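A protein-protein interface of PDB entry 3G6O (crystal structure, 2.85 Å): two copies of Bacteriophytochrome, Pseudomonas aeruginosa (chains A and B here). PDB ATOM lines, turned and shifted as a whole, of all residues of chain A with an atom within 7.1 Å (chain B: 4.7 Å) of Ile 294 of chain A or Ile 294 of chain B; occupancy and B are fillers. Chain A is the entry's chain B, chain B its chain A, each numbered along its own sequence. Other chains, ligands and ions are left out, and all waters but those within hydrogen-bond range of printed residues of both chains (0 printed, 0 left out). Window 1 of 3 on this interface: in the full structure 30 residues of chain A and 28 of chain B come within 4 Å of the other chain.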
ATOM      1  N   PHE A 123       3.653  -0.851  20.731  1.00  0.00           N
ATOM      2  CA  PHE A 123       5.079  -0.615  20.566  1.00  0.00           C
ATOM      3  C   PHE A 123       5.764  -0.633  21.935  1.00  0.00           C
ATOM      4  O   PHE A 123       6.666  -1.437  22.179  1.00  0.00           O
ATOM      5  CB  PHE A 123       5.295   0.723  19.853  1.00  0.00           C
ATOM      6  CG  PHE A 123       6.718   1.181  19.829  1.00  0.00           C
ATOM      7  CD1 PHE A 123       7.560   0.825  18.790  1.00  0.00           C
ATOM      8  CD2 PHE A 123       7.204   1.996  20.838  1.00  0.00           C
ATOM      9  CE1 PHE A 123       8.869   1.254  18.768  1.00  0.00           C
ATOM     10  CE2 PHE A 123       8.512   2.428  20.825  1.00  0.00           C
ATOM     11  CZ  PHE A 123       9.346   2.060  19.792  1.00  0.00           C
ATOM     12  N   THR A 124       5.308   0.227  22.839  1.00  0.00           N
ATOM     13  CA  THR A 124       5.929   0.330  24.157  1.00  0.00           C
ATOM     14  C   THR A 124       5.967  -1.002  24.910  1.00  0.00           C
ATOM     15  O   THR A 124       6.919  -1.257  25.655  1.00  0.00           O
ATOM     16  CB  THR A 124       5.253   1.405  25.042  1.00  0.00           C
ATOM     17  OG1 THR A 124       5.144   2.635  24.315  1.00  0.00           O
ATOM     18  CG2 THR A 124       6.068   1.645  26.313  1.00  0.00           C
ATOM     19  N   LEU A 125       4.957  -1.852  24.735  1.00  0.00           N
ATOM     20  CA  LEU A 125       4.979  -3.125  25.451  1.00  0.00           C
ATOM     21  C   LEU A 125       5.932  -4.142  24.826  1.00  0.00           C
ATOM     22  O   LEU A 125       6.489  -4.984  25.534  1.00  0.00           O
ATOM     23  CB  LEU A 125       3.587  -3.716  25.677  1.00  0.00           C
ATOM     24  CG  LEU A 125       3.665  -4.884  26.674  1.00  0.00           C
ATOM     25  CD1 LEU A 125       2.727  -4.711  27.862  1.00  0.00           C
ATOM     26  CD2 LEU A 125       3.448  -6.234  25.995  1.00  0.00           C
ATOM     27  N   ALA A 127       8.819  -3.095  23.470  1.00  0.00           N
ATOM     28  CA  ALA A 127       9.997  -2.534  24.109  1.00  0.00           C
ATOM     29  C   ALA A 127      10.140  -3.031  25.540  1.00  0.00           C
ATOM     30  O   ALA A 127      11.188  -3.547  25.925  1.00  0.00           O
ATOM     31  CB  ALA A 127       9.945  -1.009  24.081  1.00  0.00           C
ATOM     32  N   GLN A 128       9.079  -2.882  26.327  1.00  0.00           N
ATOM     33  CA  GLN A 128       9.160  -3.162  27.759  1.00  0.00           C
ATOM     34  C   GLN A 128       9.234  -4.649  28.082  1.00  0.00           C
ATOM     35  O   GLN A 128       9.923  -5.048  29.024  1.00  0.00           O
ATOM     36  CB  GLN A 128       8.012  -2.494  28.516  1.00  0.00           C
ATOM     37  CG  GLN A 128       8.061  -0.980  28.457  1.00  0.00           C
ATOM     38  CD  GLN A 128       7.288  -0.352  29.585  1.00  0.00           C
ATOM     39  OE1 GLN A 128       6.070  -0.184  29.503  1.00  0.00           O
ATOM     40  NE2 GLN A 128       7.993   0.007  30.654  1.00  0.00           N
ATOM     41  N   ILE A 130      10.678  -7.029  26.314  1.00  0.00           N
ATOM     42  CA  ILE A 130      12.026  -7.498  26.043  1.00  0.00           C
ATOM     43  C   ILE A 130      13.028  -6.903  27.036  1.00  0.00           C
ATOM     44  O   ILE A 130      13.909  -7.594  27.548  1.00  0.00           O
ATOM     45  CB  ILE A 130      12.419  -7.178  24.580  1.00  0.00           C
ATOM     46  CG1 ILE A 130      13.325  -8.272  24.001  1.00  0.00           C
ATOM     47  CG2 ILE A 130      12.970  -5.774  24.443  1.00  0.00           C
ATOM     48  CD1 ILE A 130      14.346  -8.820  24.962  1.00  0.00           C
ATOM     49  N   ILE A 131      12.884  -5.618  27.325  1.00  0.00           N
ATOM     50  CA  ILE A 131      13.787  -4.971  28.258  1.00  0.00           C
ATOM     51  C   ILE A 131      13.738  -5.696  29.606  1.00  0.00           C
ATOM     52  O   ILE A 131      14.758  -5.995  30.205  1.00  0.00           O
ATOM     53  CB  ILE A 131      13.447  -3.481  28.402  1.00  0.00           C
ATOM     54  CG1 ILE A 131      13.869  -2.720  27.138  1.00  0.00           C
ATOM     55  CG2 ILE A 131      14.135  -2.882  29.617  1.00  0.00           C
ATOM     56  CD1 ILE A 131      13.510  -1.236  27.152  1.00  0.00           C
ATOM     57  N   GLN A 135      16.920  -7.326  32.416  1.00  0.00           N
ATOM     58  CA  GLN A 135      17.102  -6.775  33.748  1.00  0.00           C
ATOM     59  C   GLN A 135      16.833  -7.753  34.890  1.00  0.00           C
ATOM     60  O   GLN A 135      16.959  -7.390  36.069  1.00  0.00           O
ATOM     61  CB  GLN A 135      16.261  -5.511  33.881  1.00  0.00           C
ATOM     62  CG  GLN A 135      16.437  -4.574  32.689  1.00  0.00           C
ATOM     63  CD  GLN A 135      15.757  -3.243  32.887  1.00  0.00           C
ATOM     64  OE1 GLN A 135      14.657  -3.169  33.438  1.00  0.00           O
ATOM     65  NE2 GLN A 135      16.413  -2.176  32.440  1.00  0.00           N
ATOM     66  N   PRO A 207      22.482  -0.363  15.181  1.00  0.00           N
ATOM     67  CA  PRO A 207      22.011  -1.379  16.119  1.00  0.00           C
ATOM     68  C   PRO A 207      21.583  -2.613  15.362  1.00  0.00           C
ATOM     69  O   PRO A 207      21.980  -3.734  15.680  1.00  0.00           O
ATOM     70  CB  PRO A 207      20.777  -0.723  16.739  1.00  0.00           C
ATOM     71  CG  PRO A 207      21.065   0.767  16.651  1.00  0.00           C
ATOM     72  CD  PRO A 207      21.827   0.943  15.376  1.00  0.00           C
ATOM     73  N   ILE A 208      20.802  -2.380  14.319  1.00  0.00           N
ATOM     74  CA  ILE A 208      20.015  -3.433  13.705  1.00  0.00           C
ATOM     75  C   ILE A 208      20.182  -3.569  12.193  1.00  0.00           C
ATOM     76  O   ILE A 208      20.070  -2.573  11.459  1.00  0.00           O
ATOM     77  CB  ILE A 208      18.532  -3.170  13.982  1.00  0.00           C
ATOM     78  CG1 ILE A 208      18.217  -3.461  15.445  1.00  0.00           C
ATOM     79  CG2 ILE A 208      17.659  -3.988  13.068  1.00  0.00           C
ATOM     80  CD1 ILE A 208      16.822  -3.127  15.827  1.00  0.00           C
ATOM     81  N   PRO A 287       8.805  -0.244  12.677  1.00  0.00           N
ATOM     82  CA  PRO A 287       8.439   0.131  14.045  1.00  0.00           C
ATOM     83  C   PRO A 287       8.897  -0.894  15.070  1.00  0.00           C
ATOM     84  O   PRO A 287       9.415  -0.509  16.120  1.00  0.00           O
ATOM     85  CB  PRO A 287       6.913   0.186  13.991  1.00  0.00           C
ATOM     86  CG  PRO A 287       6.591   0.385  12.556  1.00  0.00           C
ATOM     87  CD  PRO A 287       7.611  -0.419  11.835  1.00  0.00           C
ATOM     88  N   VAL A 288       8.714  -2.175  14.766  1.00  0.00           N
ATOM     89  CA  VAL A 288       9.228  -3.234  15.628  1.00  0.00           C
ATOM     90  C   VAL A 288      10.757  -3.217  15.688  1.00  0.00           C
ATOM     91  O   VAL A 288      11.341  -3.261  16.772  1.00  0.00           O
ATOM     92  CB  VAL A 288       8.768  -4.607  15.157  1.00  0.00           C
ATOM     93  CG1 VAL A 288       9.383  -5.686  16.042  1.00  0.00           C
ATOM     94  CG2 VAL A 288       7.239  -4.672  15.142  1.00  0.00           C
ATOM     95  N   ARG A 289      11.400  -3.154  14.525  1.00  0.00           N
ATOM     96  CA  ARG A 289      12.845  -2.998  14.476  1.00  0.00           C
ATOM     97  C   ARG A 289      13.219  -1.852  15.422  1.00  0.00           C
ATOM     98  O   ARG A 289      14.229  -1.912  16.120  1.00  0.00           O
ATOM     99  CB  ARG A 289      13.320  -2.699  13.051  1.00  0.00           C
ATOM    100  CG  ARG A 289      12.929  -3.765  12.042  1.00  0.00           C
ATOM    101  CD  ARG A 289      13.905  -3.813  10.864  1.00  0.00           C
ATOM    102  NE  ARG A 289      14.073  -2.518  10.201  1.00  0.00           N
ATOM    103  CZ  ARG A 289      13.238  -2.045   9.283  1.00  0.00           C
ATOM    104  NH1 ARG A 289      12.184  -2.763   8.940  1.00  0.00           N
ATOM    105  NH2 ARG A 289      13.443  -0.861   8.718  1.00  0.00           N
ATOM    106  N   MET A 290      12.379  -0.823  15.478  1.00  0.00           N
ATOM    107  CA  MET A 290      12.668   0.339  16.309  1.00  0.00           C
ATOM    108  C   MET A 290      12.461   0.088  17.796  1.00  0.00           C
ATOM    109  O   MET A 290      12.889   0.892  18.624  1.00  0.00           O
ATOM    110  CB  MET A 290      11.851   1.553  15.861  1.00  0.00           C
ATOM    111  CG  MET A 290      12.212   2.081  14.481  1.00  0.00           C
ATOM    112  SD  MET A 290      13.994   2.189  14.260  1.00  0.00           S
ATOM    113  CE  MET A 290      14.396   3.523  15.370  1.00  0.00           C
ATOM    114  N   SER A 291      11.780  -1.005  18.136  1.00  0.00           N
ATOM    115  CA  SER A 291      11.673  -1.414  19.534  1.00  0.00           C
ATOM    116  C   SER A 291      13.009  -2.030  19.888  1.00  0.00           C
ATOM    117  O   SER A 291      13.663  -1.620  20.846  1.00  0.00           O
ATOM    118  CB  SER A 291      10.588  -2.468  19.742  1.00  0.00           C
ATOM    119  OG  SER A 291       9.626  -2.462  18.703  1.00  0.00           O
ATOM    120  N   PHE A 292      13.412  -3.010  19.084  1.00  0.00           N
ATOM    121  CA  PHE A 292      14.702  -3.672  19.244  1.00  0.00           C
ATOM    122  C   PHE A 292      15.880  -2.700  19.157  1.00  0.00           C
ATOM    123  O   PHE A 292      16.916  -2.921  19.787  1.00  0.00           O
ATOM    124  CB  PHE A 292      14.871  -4.769  18.196  1.00  0.00           C
ATOM    125  CG  PHE A 292      13.771  -5.782  18.198  1.00  0.00           C
ATOM    126  CD1 PHE A 292      13.129  -6.112  19.373  1.00  0.00           C
ATOM    127  CD2 PHE A 292      13.396  -6.424  17.025  1.00  0.00           C
ATOM    128  CE1 PHE A 292      12.124  -7.048  19.384  1.00  0.00           C
ATOM    129  CE2 PHE A 292      12.394  -7.356  17.027  1.00  0.00           C
ATOM    130  CZ  PHE A 292      11.755  -7.667  18.210  1.00  0.00           C
ATOM    131  N   GLN A 293      15.742  -1.629  18.380  1.00  0.00           N
ATOM    132  CA  GLN A 293      16.808  -0.646  18.332  1.00  0.00           C
ATOM    133  C   GLN A 293      17.086  -0.161  19.729  1.00  0.00           C
ATOM    134  O   GLN A 293      18.205  -0.266  20.234  1.00  0.00           O
ATOM    135  CB  GLN A 293      16.432   0.544  17.472  1.00  0.00           C
ATOM    136  CG  GLN A 293      17.387   1.706  17.665  1.00  0.00           C
ATOM    137  CD  GLN A 293      17.488   2.584  16.432  1.00  0.00           C
ATOM    138  OE1 GLN A 293      17.232   3.792  16.491  1.00  0.00           O
ATOM    139  NE2 GLN A 293      17.846   1.977  15.299  1.00  0.00           N
ATOM    140  N   ILE A 294      16.052   0.369  20.363  1.00  0.00           N
ATOM    141  CA  ILE A 294      16.204   0.869  21.714  1.00  0.00           C
ATOM    142  C   ILE A 294      16.572  -0.231  22.711  1.00  0.00           C
ATOM    143  O   ILE A 294      17.381  -0.013  23.609  1.00  0.00           O
ATOM    144  CB  ILE A 294      14.960   1.619  22.187  1.00  0.00           C
ATOM    145  CG1 ILE A 294      14.589   1.158  23.585  1.00  0.00           C
ATOM    146  CG2 ILE A 294      13.794   1.402  21.249  1.00  0.00           C
ATOM    147  CD1 ILE A 294      13.873   2.232  24.324  1.00  0.00           C
ATOM    148  N   PHE A 295      15.975  -1.406  22.555  1.00  0.00           N
ATOM    149  CA  PHE A 295      16.380  -2.560  23.343  1.00  0.00           C
ATOM    150  C   PHE A 295      17.902  -2.657  23.300  1.00  0.00           C
ATOM    151  O   PHE A 295      18.576  -2.637  24.338  1.00  0.00           O
ATOM    152  CB  PHE A 295      15.777  -3.831  22.777  1.00  0.00           C
ATOM    153  CG  PHE A 295      16.487  -5.080  23.216  1.00  0.00           C
ATOM    154  CD1 PHE A 295      16.384  -5.531  24.524  1.00  0.00           C
ATOM    155  CD2 PHE A 295      17.258  -5.804  22.323  1.00  0.00           C
ATOM    156  CE1 PHE A 295      17.033  -6.683  24.931  1.00  0.00           C
ATOM    157  CE2 PHE A 295      17.912  -6.957  22.725  1.00  0.00           C
ATOM    158  CZ  PHE A 295      17.801  -7.396  24.029  1.00  0.00           C
ATOM    159  N   SER A 296      18.432  -2.744  22.083  1.00  0.00           N
ATOM    160  CA  SER A 296      19.877  -2.820  21.875  1.00  0.00           C
ATOM    161  C   SER A 296      20.640  -1.765  22.685  1.00  0.00           C
ATOM    162  O   SER A 296      21.662  -2.062  23.310  1.00  0.00           O
ATOM    163  CB  SER A 296      20.230  -2.693  20.396  1.00  0.00           C
ATOM    164  OG  SER A 296      21.553  -2.230  20.234  1.00  0.00           O
ATOM    165  N   GLN A 297      20.150  -0.530  22.669  1.00  0.00           N
ATOM    166  CA  GLN A 297      20.784   0.533  23.456  1.00  0.00           C
ATOM    167  C   GLN A 297      20.845   0.141  24.927  1.00  0.00           C
ATOM    168  O   GLN A 297      21.915   0.158  25.537  1.00  0.00           O
ATOM    169  CB  GLN A 297      20.040   1.866  23.293  1.00  0.00           C
ATOM    170  CG  GLN A 297      20.377   2.896  24.345  1.00  0.00           C
ATOM    171  CD  GLN A 297      19.633   4.197  24.125  1.00  0.00           C
ATOM    172  OE1 GLN A 297      18.506   4.197  23.634  1.00  0.00           O
ATOM    173  NE2 GLN A 297      20.261   5.316  24.486  1.00  0.00           N
ATOM    174  N   VAL A 298      19.689  -0.216  25.484  1.00  0.00           N
ATOM    175  CA  VAL A 298      19.595  -0.619  26.884  1.00  0.00           C
ATOM    176  C   VAL A 298      20.464  -1.821  27.203  1.00  0.00           C
ATOM    177  O   VAL A 298      21.257  -1.824  28.148  1.00  0.00           O
ATOM    178  CB  VAL A 298      18.178  -1.028  27.219  1.00  0.00           C
ATOM    179  CG1 VAL A 298      18.128  -1.593  28.605  1.00  0.00           C
ATOM    180  CG2 VAL A 298      17.261   0.169  27.120  1.00  0.00           C
ATOM    181  N   CYS A 299      20.290  -2.856  26.401  1.00  0.00           N
ATOM    182  CA  CYS A 299      21.032  -4.082  26.579  1.00  0.00           C
ATOM    183  C   CYS A 299      22.541  -3.878  26.551  1.00  0.00           C
ATOM    184  O   CYS A 299      23.269  -4.486  27.335  1.00  0.00           O
ATOM    185  CB  CYS A 299      20.632  -5.080  25.509  1.00  0.00           C
ATOM    186  SG  CYS A 299      21.652  -6.532  25.559  1.00  0.00           S
ATOM    187  N   SER A 300      23.018  -3.034  25.643  1.00  0.00           N
ATOM    188  CA  SER A 300      24.452  -2.761  25.560  1.00  0.00           C
ATOM    189  C   SER A 300      24.984  -2.184  26.855  1.00  0.00           C
ATOM    190  O   SER A 300      26.027  -2.609  27.339  1.00  0.00           O
ATOM    191  CB  SER A 300      24.764  -1.815  24.411  1.00  0.00           C
ATOM    192  OG  SER A 300      24.741  -2.521  23.196  1.00  0.00           O
ATOM    193  N   THR B 124      11.028   7.186  19.272  1.00  0.00           N
ATOM    194  CA  THR B 124      12.159   6.343  19.647  1.00  0.00           C
ATOM    195  C   THR B 124      13.375   7.149  20.115  1.00  0.00           C
ATOM    196  O   THR B 124      14.103   6.698  21.009  1.00  0.00           O
ATOM    197  CB  THR B 124      12.574   5.355  18.538  1.00  0.00           C
ATOM    198  OG1 THR B 124      11.447   4.547  18.177  1.00  0.00           O
ATOM    199  CG2 THR B 124      13.720   4.456  19.020  1.00  0.00           C
ATOM    200  N   ALA B 127      12.790   8.660  23.775  1.00  0.00           N
ATOM    201  CA  ALA B 127      13.213   7.606  24.663  1.00  0.00           C
ATOM    202  C   ALA B 127      14.734   7.545  24.698  1.00  0.00           C
ATOM    203  O   ALA B 127      15.335   7.825  25.731  1.00  0.00           O
ATOM    204  CB  ALA B 127      12.633   6.291  24.211  1.00  0.00           C
ATOM    205  N   GLN B 128      15.350   7.231  23.559  1.00  0.00           N
ATOM    206  CA  GLN B 128      16.795   6.989  23.495  1.00  0.00           C
ATOM    207  C   GLN B 128      17.633   8.170  23.994  1.00  0.00           C
ATOM    208  O   GLN B 128      18.721   7.986  24.542  1.00  0.00           O
ATOM    209  CB  GLN B 128      17.220   6.594  22.077  1.00  0.00           C
ATOM    210  CG  GLN B 128      16.628   5.268  21.620  1.00  0.00           C
ATOM    211  CD  GLN B 128      17.454   4.598  20.545  1.00  0.00           C
ATOM    212  OE1 GLN B 128      17.458   5.029  19.392  1.00  0.00           O
ATOM    213  NE2 GLN B 128      18.171   3.538  20.919  1.00  0.00           N
ATOM    214  N   ILE B 131      17.203   8.021  28.085  1.00  0.00           N
ATOM    215  CA  ILE B 131      17.886   6.800  28.511  1.00  0.00           C
ATOM    216  C   ILE B 131      19.394   7.007  28.430  1.00  0.00           C
ATOM    217  O   ILE B 131      20.134   6.728  29.363  1.00  0.00           O
ATOM    218  CB  ILE B 131      17.495   5.619  27.614  1.00  0.00           C
ATOM    219  CG1 ILE B 131      16.076   5.137  27.940  1.00  0.00           C
ATOM    220  CG2 ILE B 131      18.480   4.485  27.749  1.00  0.00           C
ATOM    221  CD1 ILE B 131      15.700   3.856  27.231  1.00  0.00           C
ATOM    222  N   MET B 290       4.360   7.962  27.543  1.00  0.00           N
ATOM    223  CA  MET B 290       4.857   6.611  27.274  1.00  0.00           C
ATOM    224  C   MET B 290       6.377   6.519  27.082  1.00  0.00           C
ATOM    225  O   MET B 290       6.976   5.524  27.463  1.00  0.00           O
ATOM    226  CB  MET B 290       4.131   5.980  26.091  1.00  0.00           C
ATOM    227  CG  MET B 290       2.628   5.915  26.267  1.00  0.00           C
ATOM    228  SD  MET B 290       2.218   5.195  27.853  1.00  0.00           S
ATOM    229  CE  MET B 290       2.775   3.519  27.612  1.00  0.00           C
ATOM    230  N   SER B 291       6.999   7.543  26.499  1.00  0.00           N
ATOM    231  CA  SER B 291       8.459   7.559  26.409  1.00  0.00           C
ATOM    232  C   SER B 291       8.968   7.400  27.814  1.00  0.00           C
ATOM    233  O   SER B 291       9.634   6.429  28.152  1.00  0.00           O
ATOM    234  CB  SER B 291       9.008   8.890  25.879  1.00  0.00           C
ATOM    235  OG  SER B 291       8.131   9.523  24.976  1.00  0.00           O
ATOM    236  N   PHE B 292       8.629   8.388  28.628  1.00  0.00           N
ATOM    237  CA  PHE B 292       9.052   8.453  30.017  1.00  0.00           C
ATOM    238  C   PHE B 292       8.550   7.282  30.848  1.00  0.00           C
ATOM    239  O   PHE B 292       9.048   7.047  31.949  1.00  0.00           O
ATOM    240  CB  PHE B 292       8.563   9.756  30.642  1.00  0.00           C
ATOM    241  CG  PHE B 292       9.053  10.983  29.934  1.00  0.00           C
ATOM    242  CD1 PHE B 292      10.396  11.141  29.664  1.00  0.00           C
ATOM    243  CD2 PHE B 292       8.176  11.970  29.543  1.00  0.00           C
ATOM    244  CE1 PHE B 292      10.858  12.265  29.018  1.00  0.00           C
ATOM    245  CE2 PHE B 292       8.634  13.086  28.897  1.00  0.00           C
ATOM    246  CZ  PHE B 292       9.977  13.234  28.632  1.00  0.00           C
ATOM    247  N   GLN B 293       7.559   6.556  30.341  1.00  0.00           N
ATOM    248  CA  GLN B 293       7.116   5.372  31.054  1.00  0.00           C
ATOM    249  C   GLN B 293       8.221   4.346  30.988  1.00  0.00           C
ATOM    250  O   GLN B 293       8.692   3.852  32.015  1.00  0.00           O
ATOM    251  CB  GLN B 293       5.841   4.791  30.467  1.00  0.00           C
ATOM    252  CG  GLN B 293       5.651   3.335  30.844  1.00  0.00           C
ATOM    253  CD  GLN B 293       4.201   2.940  30.876  1.00  0.00           C
ATOM    254  OE1 GLN B 293       3.802   1.936  30.265  1.00  0.00           O
ATOM    255  NE2 GLN B 293       3.386   3.737  31.573  1.00  0.00           N
ATOM    256  N   ILE B 294       8.651   4.046  29.769  1.00  0.00           N
ATOM    257  CA  ILE B 294       9.742   3.107  29.580  1.00  0.00           C
ATOM    258  C   ILE B 294      11.072   3.627  30.124  1.00  0.00           C
ATOM    259  O   ILE B 294      11.902   2.835  30.557  1.00  0.00           O
ATOM    260  CB  ILE B 294       9.883   2.650  28.119  1.00  0.00           C
ATOM    261  CG1 ILE B 294      11.322   2.776  27.679  1.00  0.00           C
ATOM    262  CG2 ILE B 294       8.979   3.434  27.172  1.00  0.00           C
ATOM    263  CD1 ILE B 294      11.544   2.027  26.407  1.00  0.00           C
ATOM    264  N   PHE B 295      11.271   4.940  30.139  1.00  0.00           N
ATOM    265  CA  PHE B 295      12.447   5.482  30.812  1.00  0.00           C
ATOM    266  C   PHE B 295      12.436   5.029  32.260  1.00  0.00           C
ATOM    267  O   PHE B 295      13.456   4.573  32.789  1.00  0.00           O
ATOM    268  CB  PHE B 295      12.458   7.001  30.743  1.00  0.00           C
ATOM    269  CG  PHE B 295      13.375   7.651  31.741  1.00  0.00           C
ATOM    270  CD1 PHE B 295      14.728   7.376  31.732  1.00  0.00           C
ATOM    271  CD2 PHE B 295      12.887   8.553  32.675  1.00  0.00           C
ATOM    272  CE1 PHE B 295      15.590   7.980  32.643  1.00  0.00           C
ATOM    273  CE2 PHE B 295      13.737   9.163  33.589  1.00  0.00           C
ATOM    274  CZ  PHE B 295      15.090   8.877  33.573  1.00  0.00           C
ATOM    275  N   SER B 296      11.268   5.135  32.892  1.00  0.00           N
ATOM    276  CA  SER B 296      11.125   4.754  34.296  1.00  0.00           C
ATOM    277  C   SER B 296      11.472   3.284  34.531  1.00  0.00           C
ATOM    278  O   SER B 296      12.035   2.925  35.569  1.00  0.00           O
ATOM    279  CB  SER B 296       9.719   5.048  34.810  1.00  0.00           C
ATOM    280  OG  SER B 296       9.484   4.397  36.046  1.00  0.00           O
ATOM    281  N   GLN B 297      11.141   2.427  33.572  1.00  0.00           N
ATOM    282  CA  GLN B 297      11.534   1.022  33.682  1.00  0.00           C
ATOM    283  C   GLN B 297      13.051   0.918  33.626  1.00  0.00           C
ATOM    284  O   GLN B 297      13.674   0.245  34.449  1.00  0.00           O
ATOM    285  CB  GLN B 297      10.904   0.179  32.570  1.00  0.00           C
ATOM    286  CG  GLN B 297      11.412  -1.246  32.545  1.00  0.00           C
ATOM    287  CD  GLN B 297      10.822  -2.070  31.421  1.00  0.00           C
ATOM    288  OE1 GLN B 297      10.270  -1.529  30.470  1.00  0.00           O
ATOM    289  NE2 GLN B 297      10.939  -3.389  31.530  1.00  0.00           N
ATOM    290  N   VAL B 298      13.638   1.605  32.652  1.00  0.00           N
ATOM    291  CA  VAL B 298      15.082   1.600  32.462  1.00  0.00           C
ATOM    292  C   VAL B 298      15.844   2.210  33.641  1.00  0.00           C
ATOM    293  O   VAL B 298      16.767   1.603  34.183  1.00  0.00           O
ATOM    294  CB  VAL B 298      15.461   2.339  31.180  1.00  0.00           C
ATOM    295  CG1 VAL B 298      16.913   2.134  30.892  1.00  0.00           C
ATOM    296  CG2 VAL B 298      14.637   1.814  30.030  1.00  0.00           C
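Phe 123 of chain A touches Thr 124 of chain B. Thr 124 of chain A touches Met 290 of chain B (OG1 to CB, 3.9 Å). Thr 124 of chain A touches Ile 294 of chain B (CG2 to CG2, 3.5 Å). Ile 294 of chain B touches Gln 128 of chain A (CA to NE2, 3.7 Å). CD1 of Ile 294 of chain B touches CD1 of Ile 131 of chain A (3.9 Å). Gln 135 of chain A touches Gln 297 of chain B. Gln 128 of chain B touches Ile 294 of chain A (NE2 to CA, 3.4 Å). CD1 of Ile 294 of chain A touches CD1 of Ile 131 of chain B, 3.8 Å away. CD1 of Ile 294 of chain A touches CD1 of Ile 294 of chain B, at 3.1 Å. NE2 of Gln 297 of chain A touches CG2 of Ile 131 of chain B, at 3.8 Å.
Of the 13 printed residues of chain B, 7 touch a printed residue of chain A. Of the 24 printed residues of chain A, 9 touch a printed residue of chain B. Among the printed residues, no Asp or Glu carboxylate lies within 4 Å of a Lys or Arg side-chain nitrogen of the other chain.
Of the printed residues of chain B, Ile 131 of chain A touches Ile 294 (3.9 Å) and Gln 297 (3.8 Å). Of the printed residues of chain B, Gln 135 of chain A touches Gln 297 (3.7 Å). Of the printed residues of chain B, Met 290 of chain A touches Thr 124 (3.7 Å). Ile 294 of chain A touches four residues of chain B. Ser 296 of chain A touches none of the printed residues of chain B. Printed residues of chain A within 4 Å of Thr 124 of chain B: Phe 123, Met 290 and Ile 294. Of the printed residues of chain A, Ile 294 of chain B touches Thr 124 (3.5 Å), Gln 128 (3.7 Å), Ile 131 (3.9 Å) and Ile 294 (3.1 Å). Of the printed residues of chain A, Gln 297 of chain B touches Gln 128, Ile 131 and Gln 135. The nearest residue of chain B that does not touch Ile 294 of chain A is Ala 127 of chain B (4.2 Å). The nearest residue of chain A that does not touch Ile 294 of chain B is Ala 127 of chain A (4.1 Å).
The side-chain amide oxygen of Gln 128 of chain A sits close to the side-chain amide oxygen of Gln 293 of chain B (3.2 Å). NE2 of Gln 128 of chain B is in hydrogen-bond range of OE1 of Gln 297 of chain A. OE1 of Gln 128 of chain B lies close to OE1 of Gln 293 of chain A (3.2 Å). OE1 of Gln 297 of chain B is in hydrogen-bond range of NE2 of Gln 128 of chain A, at 2.8 Å.
Thr 124 of chain A touches Ile 294 of chain B, and with the chains exchanged Ile 294 of chain A touches Thr 124 of chain B. Gln 128 of chain A touches Ile 294 of chain B, and with the chains exchanged Ile 294 of chain A touches Gln 128 of chain B. Gln 128 of chain A touches Gln 297 of chain B, and with the chains exchanged Gln 297 of chain A touches Gln 128 of chain B. Ile 131 of chain A touches Ile 294 of chain B, and with the chains exchanged Ile 294 of chain A touches Ile 131 of chain B.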
